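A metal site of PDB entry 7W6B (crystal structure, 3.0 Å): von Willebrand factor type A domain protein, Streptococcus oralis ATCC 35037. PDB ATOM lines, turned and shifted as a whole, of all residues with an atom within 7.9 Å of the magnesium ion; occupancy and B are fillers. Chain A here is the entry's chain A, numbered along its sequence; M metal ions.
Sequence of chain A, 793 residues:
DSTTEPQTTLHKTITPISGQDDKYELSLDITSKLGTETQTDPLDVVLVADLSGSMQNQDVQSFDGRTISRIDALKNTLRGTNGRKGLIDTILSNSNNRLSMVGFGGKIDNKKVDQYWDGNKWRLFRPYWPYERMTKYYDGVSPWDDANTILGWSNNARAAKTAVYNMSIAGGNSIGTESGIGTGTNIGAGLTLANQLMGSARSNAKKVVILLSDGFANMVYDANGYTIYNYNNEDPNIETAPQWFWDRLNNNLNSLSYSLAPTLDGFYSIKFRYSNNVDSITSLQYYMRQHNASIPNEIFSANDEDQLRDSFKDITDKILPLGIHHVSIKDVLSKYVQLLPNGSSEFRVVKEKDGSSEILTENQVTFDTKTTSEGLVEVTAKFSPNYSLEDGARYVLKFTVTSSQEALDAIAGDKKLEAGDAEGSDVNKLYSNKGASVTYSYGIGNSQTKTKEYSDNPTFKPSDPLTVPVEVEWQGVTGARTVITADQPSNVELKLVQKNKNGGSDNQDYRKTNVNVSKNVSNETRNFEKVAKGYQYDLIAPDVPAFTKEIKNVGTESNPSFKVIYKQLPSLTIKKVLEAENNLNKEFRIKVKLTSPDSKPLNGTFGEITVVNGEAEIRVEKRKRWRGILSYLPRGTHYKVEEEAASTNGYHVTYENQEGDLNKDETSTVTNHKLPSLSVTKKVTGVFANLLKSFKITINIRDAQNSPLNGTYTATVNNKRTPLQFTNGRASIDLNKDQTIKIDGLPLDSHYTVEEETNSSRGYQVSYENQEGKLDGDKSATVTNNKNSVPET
OD2 of Asp 214 is in salt-bridge range of NH1 of Arg 70 (3.4 Å).
The backbone NH (N) of Asp 50 lies within hydrogen-bond range of the backbone carbonyl oxygen (O) of Leu 212, 3.0 Å away.
The guanidinium group (NH1) of Arg 70 sits at hydrogen-bond distance from the backbone carbonyl oxygen (O) of Ser 54.
The backbone NH (N) of Ser 52 lies within hydrogen-bond range of the side-chain carboxylate (OD1) of Asp 50.
The side-chain amide oxygen (OD1) of Asn 218 is in hydrogen-bond range of the backbone NH (N) of Thr 185 (3.0 Å).
OD2 of Asp 214 sits close to N of Met 55 (2.9 Å).
The backbone NH (N) of Asp 214 is in hydrogen-bond range of the side-chain carboxylate (OD2) of Asp 50 (3.2 Å).
OG1 of Thr 185 touches the magnesium ion, 3.1 Å away.
Gly 215 touches the magnesium ion.
Within 4 Å of the magnesium ion: Asp 50, Ser 52, Ser 54, Thr 185, Asp 214 and Gly 215.
The nearest printed residue that does not touch the magnesium ion is Met 55 (4.6 Å).
The magnesium ion is bound by the side-chain carboxylate of Asp 214 (1.9 Å), the side-chain hydroxyl of Ser 52 (2.0 Å) and the side-chain hydroxyl of Ser 54 (2.5 Å).
Slightly farther from the magnesium ion lies the side-chain carboxylate (OD2) of Asp 50 (2.8 Å).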
ATOM      1  N   ASP A  50     -12.525  16.396  16.893  1.00  0.00           N
ATOM      2  CA  ASP A  50     -12.311  14.973  17.114  1.00  0.00           C
ATOM      3  C   ASP A  50     -11.122  14.507  16.277  1.00  0.00           C
ATOM      4  O   ASP A  50     -11.088  14.690  15.061  1.00  0.00           O
ATOM      5  CB  ASP A  50     -13.594  14.158  16.834  1.00  0.00           C
ATOM      6  CG  ASP A  50     -13.577  12.746  17.416  1.00  0.00           C
ATOM      7  OD1 ASP A  50     -12.487  12.287  17.780  1.00  0.00           O
ATOM      8  OD2 ASP A  50     -14.654  12.131  17.516  1.00  0.00           O
ATOM      9  N   LEU A  51     -10.111  13.954  16.962  1.00  0.00           N
ATOM     10  CA  LEU A  51      -8.926  13.419  16.279  1.00  0.00           C
ATOM     11  C   LEU A  51      -8.836  11.914  16.519  1.00  0.00           C
ATOM     12  O   LEU A  51      -7.742  11.335  16.442  1.00  0.00           O
ATOM     13  CB  LEU A  51      -7.681  14.151  16.788  1.00  0.00           C
ATOM     14  CG  LEU A  51      -7.391  15.510  16.167  1.00  0.00           C
ATOM     15  CD1 LEU A  51      -5.976  15.957  16.493  1.00  0.00           C
ATOM     16  CD2 LEU A  51      -7.591  15.466  14.651  1.00  0.00           C
ATOM     17  N   SER A  52      -9.988  11.295  16.810  1.00  0.00           N
ATOM     18  CA  SER A  52     -10.060   9.884  17.123  1.00  0.00           C
ATOM     19  C   SER A  52      -9.714   9.056  15.886  1.00  0.00           C
ATOM     20  O   SER A  52      -9.647   9.574  14.779  1.00  0.00           O
ATOM     21  CB  SER A  52     -11.395   9.491  17.712  1.00  0.00           C
ATOM     22  OG  SER A  52     -12.460   9.745  16.815  1.00  0.00           O
ATOM     23  N   GLY A  53      -9.504   7.754  16.117  1.00  0.00           N
ATOM     24  CA  GLY A  53      -9.155   6.805  15.062  1.00  0.00           C
ATOM     25  C   GLY A  53     -10.249   6.706  14.009  1.00  0.00           C
ATOM     26  O   GLY A  53      -9.944   6.584  12.817  1.00  0.00           O
ATOM     27  N   SER A  54     -11.509   6.788  14.461  1.00  0.00           N
ATOM     28  CA  SER A  54     -12.665   6.670  13.586  1.00  0.00           C
ATOM     29  C   SER A  54     -12.755   7.858  12.626  1.00  0.00           C
ATOM     30  O   SER A  54     -13.435   7.766  11.604  1.00  0.00           O
ATOM     31  CB  SER A  54     -13.958   6.460  14.362  1.00  0.00           C
ATOM     32  OG  SER A  54     -14.056   7.326  15.477  1.00  0.00           O
ATOM     33  N   MET A  55     -12.030   8.939  12.923  1.00  0.00           N
ATOM     34  CA  MET A  55     -12.094  10.147  12.108  1.00  0.00           C
ATOM     35  C   MET A  55     -11.117  10.077  10.932  1.00  0.00           C
ATOM     36  O   MET A  55     -10.955  11.070  10.219  1.00  0.00           O
ATOM     37  CB  MET A  55     -11.811  11.398  12.952  1.00  0.00           C
ATOM     38  N   GLN A  56     -10.484   8.916  10.740  1.00  0.00           N
ATOM     39  CA  GLN A  56      -9.652   8.693   9.563  1.00  0.00           C
ATOM     40  C   GLN A  56     -10.353   7.765   8.565  1.00  0.00           C
ATOM     41  O   GLN A  56      -9.830   7.509   7.473  1.00  0.00           O
ATOM     42  CB  GLN A  56      -8.232   8.258   9.936  1.00  0.00           C
ATOM     43  CG  GLN A  56      -7.227   8.558   8.830  1.00  0.00           C
ATOM     44  CD  GLN A  56      -5.904   9.077   9.336  1.00  0.00           C
ATOM     45  OE1 GLN A  56      -5.441  10.144   8.934  1.00  0.00           O
ATOM     46  NE2 GLN A  56      -5.285   8.325  10.233  1.00  0.00           N
ATOM     47  N   ARG A  70     -12.293  11.562   6.682  1.00  0.00           N
ATOM     48  CA  ARG A  70     -12.939  12.645   7.411  1.00  0.00           C
ATOM     49  C   ARG A  70     -11.903  13.730   7.748  1.00  0.00           C
ATOM     50  O   ARG A  70     -12.201  14.918   7.674  1.00  0.00           O
ATOM     51  CB  ARG A  70     -13.651  12.170   8.678  1.00  0.00           C
ATOM     52  CG  ARG A  70     -14.264  10.778   8.586  1.00  0.00           C
ATOM     53  CD  ARG A  70     -15.072  10.428   9.825  1.00  0.00           C
ATOM     54  NE  ARG A  70     -16.089   9.410   9.554  1.00  0.00           N
ATOM     55  CZ  ARG A  70     -16.589   8.575  10.461  1.00  0.00           C
ATOM     56  NH1 ARG A  70     -16.160   8.609  11.715  1.00  0.00           N
ATOM     57  NH2 ARG A  70     -17.505   7.693  10.114  1.00  0.00           N
ATOM     58  N   PHE A 104      -8.780  16.476  19.997  1.00  0.00           N
ATOM     59  CA  PHE A 104      -8.966  15.579  21.133  1.00  0.00           C
ATOM     60  C   PHE A 104      -8.927  14.114  20.694  1.00  0.00           C
ATOM     61  O   PHE A 104      -9.481  13.757  19.647  1.00  0.00           O
ATOM     62  CB  PHE A 104     -10.197  15.974  21.945  1.00  0.00           C
ATOM     63  CG  PHE A 104     -11.556  15.613  21.385  1.00  0.00           C
ATOM     64  CD1 PHE A 104     -12.046  14.312  21.471  1.00  0.00           C
ATOM     65  CD2 PHE A 104     -12.376  16.585  20.849  1.00  0.00           C
ATOM     66  CE1 PHE A 104     -13.307  13.992  20.973  1.00  0.00           C
ATOM     67  CE2 PHE A 104     -13.634  16.261  20.360  1.00  0.00           C
ATOM     68  CZ  PHE A 104     -14.098  14.962  20.427  1.00  0.00           C
ATOM     69  N   THR A 183      -6.424   7.340  20.198  1.00  0.00           N
ATOM     70  CA  THR A 183      -7.312   7.046  19.072  1.00  0.00           C
ATOM     71  C   THR A 183      -8.764   6.931  19.549  1.00  0.00           C
ATOM     72  O   THR A 183      -9.658   6.690  18.743  1.00  0.00           O
ATOM     73  CB  THR A 183      -6.861   5.783  18.320  1.00  0.00           C
ATOM     74  OG1 THR A 183      -6.648   4.757  19.283  1.00  0.00           O
ATOM     75  CG2 THR A 183      -5.604   5.971  17.496  1.00  0.00           C
ATOM     76  N   GLY A 184      -8.983   7.102  20.848  1.00  0.00           N
ATOM     77  CA  GLY A 184     -10.324   7.048  21.417  1.00  0.00           C
ATOM     78  C   GLY A 184     -11.004   8.410  21.404  1.00  0.00           C
ATOM     79  O   GLY A 184     -10.369   9.420  21.103  1.00  0.00           O
ATOM     80  N   THR A 185     -12.289   8.426  21.766  1.00  0.00           N
ATOM     81  CA  THR A 185     -13.077   9.641  21.825  1.00  0.00           C
ATOM     82  C   THR A 185     -13.229  10.086  23.282  1.00  0.00           C
ATOM     83  O   THR A 185     -14.079   9.572  24.010  1.00  0.00           O
ATOM     84  CB  THR A 185     -14.423   9.439  21.100  1.00  0.00           C
ATOM     85  OG1 THR A 185     -14.193   8.761  19.868  1.00  0.00           O
ATOM     86  CG2 THR A 185     -15.162  10.742  20.845  1.00  0.00           C
ATOM     87  N   ASN A 186     -12.379  11.024  23.719  1.00  0.00           N
ATOM     88  CA  ASN A 186     -12.553  11.624  25.032  1.00  0.00           C
ATOM     89  C   ASN A 186     -12.955  13.080  24.846  1.00  0.00           C
ATOM     90  O   ASN A 186     -12.111  13.963  24.906  1.00  0.00           O
ATOM     91  CB  ASN A 186     -11.310  11.444  25.911  1.00  0.00           C
ATOM     92  CG  ASN A 186     -11.489  11.866  27.364  1.00  0.00           C
ATOM     93  OD1 ASN A 186     -12.526  12.401  27.757  1.00  0.00           O
ATOM     94  ND2 ASN A 186     -10.476  11.622  28.177  1.00  0.00           N
ATOM     95  N   LEU A 212     -16.688  19.385  17.130  1.00  0.00           N
ATOM     96  CA  LEU A 212     -16.842  18.448  16.036  1.00  0.00           C
ATOM     97  C   LEU A 212     -16.519  17.048  16.546  1.00  0.00           C
ATOM     98  O   LEU A 212     -15.453  16.842  17.110  1.00  0.00           O
ATOM     99  CB  LEU A 212     -15.897  18.843  14.897  1.00  0.00           C
ATOM    100  CG  LEU A 212     -15.888  17.908  13.689  1.00  0.00           C
ATOM    101  CD1 LEU A 212     -17.249  17.852  12.992  1.00  0.00           C
ATOM    102  CD2 LEU A 212     -14.812  18.331  12.700  1.00  0.00           C
ATOM    103  N   SER A 213     -17.440  16.110  16.312  1.00  0.00           N
ATOM    104  CA  SER A 213     -17.275  14.731  16.743  1.00  0.00           C
ATOM    105  C   SER A 213     -17.735  13.789  15.631  1.00  0.00           C
ATOM    106  O   SER A 213     -18.478  14.200  14.738  1.00  0.00           O
ATOM    107  CB  SER A 213     -18.042  14.469  18.019  1.00  0.00           C
ATOM    108  N   ASP A 214     -17.296  12.526  15.698  1.00  0.00           N
ATOM    109  CA  ASP A 214     -17.651  11.565  14.672  1.00  0.00           C
ATOM    110  C   ASP A 214     -18.328  10.340  15.285  1.00  0.00           C
ATOM    111  O   ASP A 214     -18.911   9.535  14.569  1.00  0.00           O
ATOM    112  CB  ASP A 214     -16.453  11.239  13.779  1.00  0.00           C
ATOM    113  CG  ASP A 214     -15.254  10.717  14.539  1.00  0.00           C
ATOM    114  OD1 ASP A 214     -15.336  10.578  15.771  1.00  0.00           O
ATOM    115  OD2 ASP A 214     -14.253  10.435  13.894  1.00  0.00           O
ATOM    116  N   GLY A 215     -18.258  10.228  16.613  1.00  0.00           N
ATOM    117  CA  GLY A 215     -18.823   9.105  17.365  1.00  0.00           C
ATOM    118  C   GLY A 215     -18.971   9.457  18.840  1.00  0.00           C
ATOM    119  O   GLY A 215     -18.590  10.547  19.247  1.00  0.00           O
ATOM    120  N   PHE A 216     -19.530   8.521  19.613  1.00  0.00           N
ATOM    121  CA  PHE A 216     -19.819   8.737  21.022  1.00  0.00           C
ATOM    122  C   PHE A 216     -18.538   8.623  21.854  1.00  0.00           C
ATOM    123  O   PHE A 216     -17.583   7.947  21.468  1.00  0.00           O
ATOM    124  CB  PHE A 216     -20.872   7.748  21.536  1.00  0.00           C
ATOM    125  N   ALA A 217     -18.551   9.292  23.018  1.00  0.00           N
ATOM    126  CA  ALA A 217     -17.388   9.417  23.883  1.00  0.00           C
ATOM    127  C   ALA A 217     -17.200   8.153  24.731  1.00  0.00           C
ATOM    128  O   ALA A 217     -17.893   7.940  25.721  1.00  0.00           O
ATOM    129  CB  ALA A 217     -17.480  10.665  24.733  1.00  0.00           C
ATOM    130  N   ASN A 218     -16.210   7.357  24.337  1.00  0.00           N
ATOM    131  CA  ASN A 218     -15.970   6.068  24.961  1.00  0.00           C
ATOM    132  C   ASN A 218     -14.989   6.183  26.145  1.00  0.00           C
ATOM    133  O   ASN A 218     -14.638   5.175  26.748  1.00  0.00           O
ATOM    134  CB  ASN A 218     -15.561   5.005  23.929  1.00  0.00           C
ATOM    135  CG  ASN A 218     -14.374   5.383  23.069  1.00  0.00           C
ATOM    136  OD1 ASN A 218     -13.645   6.318  23.378  1.00  0.00           O
ATOM    137  ND2 ASN A 218     -14.171   4.670  21.970  1.00  0.00           N
ATOM    138  N   PHE A 272     -20.347  15.281  12.497  1.00  0.00           N
ATOM    139  CA  PHE A 272     -19.943  14.678  11.224  1.00  0.00           C
ATOM    140  C   PHE A 272     -20.068  13.147  11.319  1.00  0.00           C
ATOM    141  O   PHE A 272     -19.547  12.543  12.249  1.00  0.00           O
ATOM    142  CB  PHE A 272     -18.510  15.085  10.861  1.00  0.00           C
ATOM    143  N   ARG A 273     -20.771  12.551  10.354  1.00  0.00           N
ATOM    144  CA  ARG A 273     -20.880  11.104  10.215  1.00  0.00           C
ATOM    145  C   ARG A 273     -21.130  10.413  11.562  1.00  0.00           C
ATOM    146  O   ARG A 273     -20.471   9.433  11.872  1.00  0.00           O
ATOM    147  CB  ARG A 273     -19.586  10.537   9.621  1.00  0.00           C
ATOM    148  CG  ARG A 273     -18.983  11.324   8.460  1.00  0.00           C
ATOM    149  CD  ARG A 273     -19.590  10.964   7.117  1.00  0.00           C
ATOM    150  NE  ARG A 273     -19.729   9.527   6.898  1.00  0.00           N
ATOM    151  CZ  ARG A 273     -20.874   8.896   6.664  1.00  0.00           C
ATOM    152  NH1 ARG A 273     -22.007   9.579   6.622  1.00  0.00           N
ATOM    153  NH2 ARG A 273     -20.879   7.593   6.476  1.00  0.00           N
HETATM  154 MG    MG M   1     -14.405   9.389  16.841  1.00  0.00          MG
